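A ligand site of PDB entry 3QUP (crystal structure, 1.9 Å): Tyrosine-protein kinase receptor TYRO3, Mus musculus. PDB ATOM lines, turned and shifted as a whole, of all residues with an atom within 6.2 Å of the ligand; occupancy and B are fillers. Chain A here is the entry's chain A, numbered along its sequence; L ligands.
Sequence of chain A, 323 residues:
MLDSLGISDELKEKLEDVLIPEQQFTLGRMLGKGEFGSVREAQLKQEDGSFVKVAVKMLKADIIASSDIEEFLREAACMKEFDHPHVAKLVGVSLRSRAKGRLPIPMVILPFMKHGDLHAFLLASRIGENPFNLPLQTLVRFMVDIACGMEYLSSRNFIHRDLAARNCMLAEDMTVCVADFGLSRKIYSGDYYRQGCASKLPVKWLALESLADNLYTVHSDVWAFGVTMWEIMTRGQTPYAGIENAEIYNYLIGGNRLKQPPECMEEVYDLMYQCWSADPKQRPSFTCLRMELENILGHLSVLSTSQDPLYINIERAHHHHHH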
ATOM      1  N   ARG A  29      34.625  22.441  14.327  1.00  0.00           N
ATOM      2  CA  ARG A  29      34.489  20.988  14.500  1.00  0.00           C
ATOM      3  C   ARG A  29      33.804  20.331  13.294  1.00  0.00           C
ATOM      4  O   ARG A  29      32.981  20.946  12.624  1.00  0.00           O
ATOM      5  CB  ARG A  29      33.759  20.640  15.813  1.00  0.00           C
ATOM      6  CG  ARG A  29      32.224  20.505  15.713  1.00  0.00           C
ATOM      7  CD  ARG A  29      31.578  20.101  17.038  1.00  0.00           C
ATOM      8  NE  ARG A  29      30.409  19.235  16.865  1.00  0.00           N
ATOM      9  CZ  ARG A  29      29.143  19.572  17.143  1.00  0.00           C
ATOM     10  NH1 ARG A  29      28.162  18.692  16.954  1.00  0.00           N
ATOM     11  NH2 ARG A  29      28.854  20.781  17.622  1.00  0.00           N
ATOM     12  N   LEU A  31      31.075  18.145  11.731  1.00  0.00           N
ATOM     13  CA  LEU A  31      29.702  17.793  12.078  1.00  0.00           C
ATOM     14  C   LEU A  31      29.284  16.446  11.479  1.00  0.00           C
ATOM     15  O   LEU A  31      28.587  15.667  12.114  1.00  0.00           O
ATOM     16  CB  LEU A  31      28.733  18.903  11.653  1.00  0.00           C
ATOM     17  CG  LEU A  31      28.748  20.246  12.394  1.00  0.00           C
ATOM     18  CD1 LEU A  31      27.910  21.281  11.668  1.00  0.00           C
ATOM     19  CD2 LEU A  31      28.283  20.110  13.825  1.00  0.00           C
ATOM     20  N   GLY A  32      29.710  16.185  10.250  1.00  0.00           N
ATOM     21  CA  GLY A  32      29.413  14.915   9.588  1.00  0.00           C
ATOM     22  C   GLY A  32      30.052  14.834   8.220  1.00  0.00           C
ATOM     23  O   GLY A  32      30.629  15.817   7.742  1.00  0.00           O
ATOM     24  N   PHE A  36      28.445  13.183  -0.688  1.00  0.00           N
ATOM     25  CA  PHE A  36      28.310  14.621  -1.005  1.00  0.00           C
ATOM     26  C   PHE A  36      29.498  15.462  -0.527  1.00  0.00           C
ATOM     27  O   PHE A  36      29.681  16.592  -0.978  1.00  0.00           O
ATOM     28  CB  PHE A  36      27.018  15.171  -0.384  1.00  0.00           C
ATOM     29  CG  PHE A  36      27.041  15.203   1.124  1.00  0.00           C
ATOM     30  CD1 PHE A  36      27.340  16.384   1.797  1.00  0.00           C
ATOM     31  CD2 PHE A  36      26.772  14.049   1.863  1.00  0.00           C
ATOM     32  CE1 PHE A  36      27.366  16.413   3.200  1.00  0.00           C
ATOM     33  CE2 PHE A  36      26.799  14.074   3.253  1.00  0.00           C
ATOM     34  CZ  PHE A  36      27.099  15.255   3.926  1.00  0.00           C
ATOM     35  N   VAL A  39      30.583  18.163   6.345  1.00  0.00           N
ATOM     36  CA  VAL A  39      30.000  19.361   6.931  1.00  0.00           C
ATOM     37  C   VAL A  39      30.728  19.667   8.231  1.00  0.00           C
ATOM     38  O   VAL A  39      30.993  18.779   9.038  1.00  0.00           O
ATOM     39  CB  VAL A  39      28.487  19.184   7.256  1.00  0.00           C
ATOM     40  CG1 VAL A  39      27.871  20.493   7.739  1.00  0.00           C
ATOM     41  CG2 VAL A  39      27.734  18.671   6.030  1.00  0.00           C
ATOM     42  N   VAL A  54      27.159  28.552  12.316  1.00  0.00           N
ATOM     43  CA  VAL A  54      26.553  28.028  11.083  1.00  0.00           C
ATOM     44  C   VAL A  54      27.021  26.611  10.771  1.00  0.00           C
ATOM     45  O   VAL A  54      27.937  26.094  11.399  1.00  0.00           O
ATOM     46  CB  VAL A  54      26.828  28.935   9.853  1.00  0.00           C
ATOM     47  CG1 VAL A  54      26.238  30.328  10.036  1.00  0.00           C
ATOM     48  CG2 VAL A  54      28.316  28.967   9.504  1.00  0.00           C
ATOM     49  N   ALA A  55      26.392  25.995   9.767  1.00  0.00           N
ATOM     50  CA  ALA A  55      26.860  24.739   9.222  1.00  0.00           C
ATOM     51  C   ALA A  55      27.467  25.055   7.858  1.00  0.00           C
ATOM     52  O   ALA A  55      26.942  25.879   7.106  1.00  0.00           O
ATOM     53  CB  ALA A  55      25.723  23.745   9.092  1.00  0.00           C
ATOM     54  N   LYS A  57      28.865  23.297   4.365  1.00  0.00           N
ATOM     55  CA  LYS A  57      28.881  22.110   3.546  1.00  0.00           C
ATOM     56  C   LYS A  57      30.084  22.121   2.600  1.00  0.00           C
ATOM     57  O   LYS A  57      30.248  23.063   1.823  1.00  0.00           O
ATOM     58  CB  LYS A  57      27.565  22.038   2.747  1.00  0.00           C
ATOM     59  CG  LYS A  57      27.001  20.646   2.552  1.00  0.00           C
ATOM     60  CD  LYS A  57      25.646  20.701   1.839  1.00  0.00           C
ATOM     61  CE  LYS A  57      25.223  19.317   1.358  1.00  0.00           C
ATOM     62  NZ  LYS A  57      23.859  19.337   0.755  1.00  0.00           N
ATOM     63  N   ALA A  88      14.686  25.219   4.417  1.00  0.00           N
ATOM     64  CA  ALA A  88      15.915  25.719   5.016  1.00  0.00           C
ATOM     65  C   ALA A  88      16.440  26.933   4.246  1.00  0.00           C
ATOM     66  O   ALA A  88      16.548  26.920   2.998  1.00  0.00           O
ATOM     67  CB  ALA A  88      16.984  24.622   5.120  1.00  0.00           C
ATOM     68  N   LYS A  89      16.723  28.001   4.989  1.00  0.00           N
ATOM     69  CA  LYS A  89      17.276  29.212   4.433  1.00  0.00           C
ATOM     70  C   LYS A  89      18.677  28.893   3.933  1.00  0.00           C
ATOM     71  O   LYS A  89      19.325  27.955   4.435  1.00  0.00           O
ATOM     72  CB  LYS A  89      17.350  30.300   5.514  1.00  0.00           C
ATOM     73  CG  LYS A  89      15.999  30.880   5.908  1.00  0.00           C
ATOM     74  CD  LYS A  89      16.038  31.616   7.258  1.00  0.00           C
ATOM     75  CE  LYS A  89      14.643  31.664   7.880  1.00  0.00           C
ATOM     76  NZ  LYS A  89      14.403  32.944   8.593  1.00  0.00           N
ATOM     77  N   LEU A 110      25.014  27.538   5.774  1.00  0.00           N
ATOM     78  CA  LEU A 110      23.646  27.263   6.207  1.00  0.00           C
ATOM     79  C   LEU A 110      23.455  27.595   7.693  1.00  0.00           C
ATOM     80  O   LEU A 110      24.418  27.472   8.468  1.00  0.00           O
ATOM     81  CB  LEU A 110      23.357  25.753   6.063  1.00  0.00           C
ATOM     82  CG  LEU A 110      23.105  24.942   4.798  1.00  0.00           C
ATOM     83  CD1 LEU A 110      22.567  25.774   3.642  1.00  0.00           C
ATOM     84  CD2 LEU A 110      24.346  24.140   4.424  1.00  0.00           C
ATOM     85  N   PRO A 111      22.220  27.953   8.110  1.00  0.00           N
ATOM     86  CA  PRO A 111      22.010  28.173   9.553  1.00  0.00           C
ATOM     87  C   PRO A 111      22.233  26.869  10.320  1.00  0.00           C
ATOM     88  O   PRO A 111      21.850  25.796   9.819  1.00  0.00           O
ATOM     89  CB  PRO A 111      20.560  28.647   9.660  1.00  0.00           C
ATOM     90  CG  PRO A 111      20.025  28.745   8.244  1.00  0.00           C
ATOM     91  CD  PRO A 111      20.952  27.961   7.353  1.00  0.00           C
ATOM     92  N   PHE A 112      22.860  26.951  11.497  1.00  0.00           N
ATOM     93  CA  PHE A 112      23.128  25.750  12.267  1.00  0.00           C
ATOM     94  C   PHE A 112      21.825  25.305  12.934  1.00  0.00           C
ATOM     95  O   PHE A 112      21.219  26.066  13.694  1.00  0.00           O
ATOM     96  CB  PHE A 112      24.242  25.930  13.321  1.00  0.00           C
ATOM     97  CG  PHE A 112      24.541  24.666  14.094  1.00  0.00           C
ATOM     98  CD1 PHE A 112      25.199  23.593  13.491  1.00  0.00           C
ATOM     99  CD2 PHE A 112      24.133  24.529  15.417  1.00  0.00           C
ATOM    100  CE1 PHE A 112      25.461  22.411  14.201  1.00  0.00           C
ATOM    101  CE2 PHE A 112      24.394  23.352  16.140  1.00  0.00           C
ATOM    102  CZ  PHE A 112      25.050  22.295  15.531  1.00  0.00           C
ATOM    103  N   MET A 113      21.403  24.090  12.634  1.00  0.00           N
ATOM    104  CA  MET A 113      20.179  23.555  13.226  1.00  0.00           C
ATOM    105  C   MET A 113      20.529  22.414  14.156  1.00  0.00           C
ATOM    106  O   MET A 113      20.755  21.280  13.705  1.00  0.00           O
ATOM    107  CB  MET A 113      19.200  23.141  12.126  1.00  0.00           C
ATOM    108  CG  MET A 113      18.848  24.293  11.178  1.00  0.00           C
ATOM    109  SD  MET A 113      17.817  23.788   9.760  1.00  0.00           S
ATOM    110  CE  MET A 113      16.343  23.389  10.683  1.00  0.00           C
ATOM    111  N   LYS A 114      20.573  22.724  15.451  1.00  0.00           N
ATOM    112  CA  LYS A 114      21.079  21.780  16.456  1.00  0.00           C
ATOM    113  C   LYS A 114      20.320  20.472  16.562  1.00  0.00           C
ATOM    114  O   LYS A 114      20.917  19.447  16.873  1.00  0.00           O
ATOM    115  CB  LYS A 114      21.159  22.462  17.830  1.00  0.00           C
ATOM    116  CG  LYS A 114      19.818  22.920  18.360  1.00  0.00           C
ATOM    117  CD  LYS A 114      20.020  23.808  19.600  1.00  0.00           C
ATOM    118  CE  LYS A 114      18.680  24.255  20.149  1.00  0.00           C
ATOM    119  NZ  LYS A 114      18.869  24.867  21.474  1.00  0.00           N
ATOM    120  N   HIS A 115      19.020  20.484  16.292  1.00  0.00           N
ATOM    121  CA  HIS A 115      18.206  19.260  16.378  1.00  0.00           C
ATOM    122  C   HIS A 115      18.509  18.226  15.285  1.00  0.00           C
ATOM    123  O   HIS A 115      17.993  17.106  15.342  1.00  0.00           O
ATOM    124  CB  HIS A 115      16.717  19.572  16.450  1.00  0.00           C
ATOM    125  CG  HIS A 115      16.348  20.341  17.679  1.00  0.00           C
ATOM    126  ND1 HIS A 115      15.435  21.385  17.668  1.00  0.00           N
ATOM    127  CD2 HIS A 115      16.810  20.252  18.950  1.00  0.00           C
ATOM    128  CE1 HIS A 115      15.323  21.874  18.892  1.00  0.00           C
ATOM    129  NE2 HIS A 115      16.158  21.219  19.683  1.00  0.00           N
ATOM    130  N   GLY A 116      19.351  18.593  14.322  1.00  0.00           N
ATOM    131  CA  GLY A 116      19.714  17.725  13.197  1.00  0.00           C
ATOM    132  C   GLY A 116      18.569  17.338  12.254  1.00  0.00           C
ATOM    133  O   GLY A 116      17.496  17.980  12.218  1.00  0.00           O
ATOM    134  N   ASP A 117      18.790  16.253  11.521  1.00  0.00           N
ATOM    135  CA  ASP A 117      17.829  15.813  10.508  1.00  0.00           C
ATOM    136  C   ASP A 117      16.755  14.883  11.016  1.00  0.00           C
ATOM    137  O   ASP A 117      16.909  14.210  12.060  1.00  0.00           O
ATOM    138  CB  ASP A 117      18.553  15.262   9.229  1.00  0.00           C
ATOM    139  CG  ASP A 117      19.108  13.830   9.420  1.00  0.00           C
ATOM    140  OD1 ASP A 117      18.341  12.873   9.518  1.00  0.00           O
ATOM    141  OD2 ASP A 117      20.337  13.653   9.466  1.00  0.00           O
ATOM    142  N   ARG A 166      16.250  12.101   5.588  1.00  0.00           N
ATOM    143  CA  ARG A 166      17.614  12.523   5.893  1.00  0.00           C
ATOM    144  C   ARG A 166      17.877  13.953   5.423  1.00  0.00           C
ATOM    145  O   ARG A 166      18.783  14.619   5.903  1.00  0.00           O
ATOM    146  CB  ARG A 166      18.671  11.543   5.289  1.00  0.00           C
ATOM    147  CG  ARG A 166      18.655  11.598   3.743  1.00  0.00           C
ATOM    148  CD  ARG A 166      19.727  10.689   3.023  1.00  0.00           C
ATOM    149  NE  ARG A 166      19.385  10.648   1.590  1.00  0.00           N
ATOM    150  CZ  ARG A 166      18.509   9.810   1.039  1.00  0.00           C
ATOM    151  NH1 ARG A 166      17.904   8.894   1.754  1.00  0.00           N
ATOM    152  NH2 ARG A 166      18.228   9.908  -0.251  1.00  0.00           N
ATOM    153  N   ASN A 167      17.086  14.438   4.463  1.00  0.00           N
ATOM    154  CA  ASN A 167      17.305  15.768   3.897  1.00  0.00           C
ATOM    155  C   ASN A 167      16.269  16.788   4.398  1.00  0.00           C
ATOM    156  O   ASN A 167      16.106  17.875   3.843  1.00  0.00           O
ATOM    157  CB  ASN A 167      17.324  15.685   2.366  1.00  0.00           C
ATOM    158  CG  ASN A 167      18.601  15.064   1.860  1.00  0.00           C
ATOM    159  OD1 ASN A 167      19.683  15.271   2.455  1.00  0.00           O
ATOM    160  ND2 ASN A 167      18.502  14.336   0.736  1.00  0.00           N
ATOM    161  N   CYS A 168      15.578  16.419   5.457  1.00  0.00           N
ATOM    162  CA  CYS A 168      14.650  17.333   6.164  1.00  0.00           C
ATOM    163  C   CYS A 168      15.267  17.652   7.510  1.00  0.00           C
ATOM    164  O   CYS A 168      15.700  16.738   8.227  1.00  0.00           O
ATOM    165  CB  CYS A 168      13.290  16.645   6.326  1.00  0.00           C
ATOM    166  SG  CYS A 168      12.466  16.437   4.733  1.00  0.00           S
ATOM    167  N   MET A 169      15.326  18.928   7.857  1.00  0.00           N
ATOM    168  CA  MET A 169      15.985  19.325   9.110  1.00  0.00           C
ATOM    169  C   MET A 169      14.933  19.718  10.156  1.00  0.00           C
ATOM    170  O   MET A 169      13.860  20.196   9.802  1.00  0.00           O
ATOM    171  CB  MET A 169      16.970  20.466   8.850  1.00  0.00           C
ATOM    172  CG  MET A 169      18.135  20.126   7.945  1.00  0.00           C
ATOM    173  SD  MET A 169      19.195  18.852   8.627  1.00  0.00           S
ATOM    174  CE  MET A 169      19.899  19.737  10.030  1.00  0.00           C
ATOM    175  N   ALA A 179      15.515  20.610   3.022  1.00  0.00           N
ATOM    176  CA  ALA A 179      16.892  21.089   2.877  1.00  0.00           C
ATOM    177  C   ALA A 179      17.609  20.309   1.772  1.00  0.00           C
ATOM    178  O   ALA A 179      17.032  19.363   1.194  1.00  0.00           O
ATOM    179  CB  ALA A 179      17.641  20.916   4.203  1.00  0.00           C
ATOM    180  N   ASP A 180      18.871  20.666   1.549  1.00  0.00           N
ATOM    181  CA  ASP A 180      19.801  19.907   0.710  1.00  0.00           C
ATOM    182  C   ASP A 180      19.235  19.813  -0.707  1.00  0.00           C
ATOM    183  O   ASP A 180      18.788  18.747  -1.162  1.00  0.00           O
ATOM    184  CB  ASP A 180      20.083  18.521   1.300  1.00  0.00           C
ATOM    185  CG  ASP A 180      20.817  18.578   2.646  1.00  0.00           C
ATOM    186  OD1 ASP A 180      21.982  19.041   2.694  1.00  0.00           O
ATOM    187  OD2 ASP A 180      20.236  18.153   3.660  1.00  0.00           O
HETATM  188  C1  LIG L   1      22.611  20.054   6.710  1.00  0.00           C
HETATM  189  C2  LIG L   1      21.787  21.301   6.753  1.00  0.00           C
HETATM  190  C3  LIG L   1      23.193  20.024   8.121  1.00  0.00           C
HETATM  191  C4  LIG L   1      21.852  18.765   6.454  1.00  0.00           C
HETATM  192  C5  LIG L   1      23.688  20.133   5.683  1.00  0.00           C
HETATM  193  C6  LIG L   1      21.935  21.951   7.947  1.00  0.00           C
HETATM  194  C7  LIG L   1      20.944  21.825   5.782  1.00  0.00           C
HETATM  195  N1  LIG L   1      22.810  21.252   8.788  1.00  0.00           N
HETATM  196  N2  LIG L   1      22.640  18.019   5.425  1.00  0.00           N
HETATM  197  C8  LIG L   1      23.906  18.733   5.155  1.00  0.00           C
HETATM  198  C9  LIG L   1      21.267  23.124   8.226  1.00  0.00           C
HETATM  199  C10 LIG L   1      20.268  23.003   6.043  1.00  0.00           C
HETATM  200  C11 LIG L   1      22.828  21.481  10.178  1.00  0.00           C
HETATM  201  C12 LIG L   1      22.816  16.566   5.684  1.00  0.00           C
HETATM  202  C13 LIG L   1      20.422  23.639   7.265  1.00  0.00           C
HETATM  203  C14 LIG L   1      23.338  20.482  11.054  1.00  0.00           C
HETATM  204  O1  LIG L   1      22.393  22.519  10.662  1.00  0.00           O
HETATM  205  C15 LIG L   1      23.539  15.908   4.504  1.00  0.00           C
HETATM  206  C16 LIG L   1      21.436  15.945   5.736  1.00  0.00           C
HETATM  207  C17 LIG L   1      24.241  19.438  10.921  1.00  0.00           C
HETATM  208  N3  LIG L   1      22.928  20.429  12.353  1.00  0.00           N
HETATM  209  C18 LIG L   1      23.576  14.402   4.680  1.00  0.00           C
HETATM  210  N4  LIG L   1      21.526  14.510   5.996  1.00  0.00           N
HETATM  211  C19 LIG L   1      24.354  18.761  12.167  1.00  0.00           C
HETATM  212  C20 LIG L   1      23.507  19.412  13.052  1.00  0.00           C
HETATM  213  C21 LIG L   1      22.166  13.848   4.856  1.00  0.00           C
HETATM  214  C22 LIG L   1      25.080  17.664  12.612  1.00  0.00           C
HETATM  215  C23 LIG L   1      23.323  19.044  14.364  1.00  0.00           C
HETATM  216  C24 LIG L   1      24.918  17.291  13.936  1.00  0.00           C
HETATM  217  C25 LIG L   1      24.068  17.965  14.782  1.00  0.00           C
HETATM  218  F1  LIG L   1      25.620  16.232  14.426  1.00  0.00           F
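The backbone NH (N) of Met 113 lies within hydrogen-bond range of an oxygen (O1) of the ligand (2.7 Å). N3 of the ligand sits at hydrogen-bond distance from O of Met 113 (2.7 Å). The backbone carbonyl oxygen (O) of Arg 166 sits at hydrogen-bond distance from a nitrogen (N4) of the ligand. The side-chain carboxylate of Asp 180 lies within salt-bridge range of a nitrogen (N2) of the ligand. The side-chain carboxylate (OD2) of Asp 117 is in salt-bridge range of a nitrogen (N4) of the ligand (3.8 Å).
The side-chain amide oxygen (OD1) of Asn 167 sits close to the side-chain carboxylate (OD2) of Asp 180, at 3.2 Å. OD1 of Asp 180 lies within salt-bridge range of NZ of Lys 57 (2.7 Å). The backbone NH (N) of Ala 55 lies within hydrogen-bond range of the backbone carbonyl oxygen (O) of Leu 110 (2.8 Å). N of Ala 179 lies within hydrogen-bond range of O of Asn 167, at 2.9 Å. N of Leu 31 sits at hydrogen-bond distance from O of Val 39 (2.8 Å). O of Gly 32 lies within hydrogen-bond range of N of Val 39 (2.7 Å).
O of Pro 111 sits close to O1 of the ligand, at 3.4 Å. Leu 31 touches the ligand (O to F1, 3.8 Å). Phe 36 touches the ligand (CE2 to C18, 3.5 Å). CG2 of Val 39 touches C8 of the ligand (3.9 Å). CB of Ala 55 touches C11 of the ligand (3.8 Å). Ala 88 touches the ligand. Leu 110 touches the ligand (CG to C10, 3.7 Å). Phe 112 touches the ligand (C to O1, 3.6 Å). O of Lys 114 touches C23 of the ligand, at 3.5 Å. Gly 116 touches the ligand (N to C23, 3.998 Å). OD1 of Asn 167 touches C21 of the ligand, 3.7 Å away. Met 169 touches the ligand. CB of Ala 179 touches C7 of the ligand, at 3.8 Å. Of the 24 residues printed, 17 come within 4 Å of the ligand.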
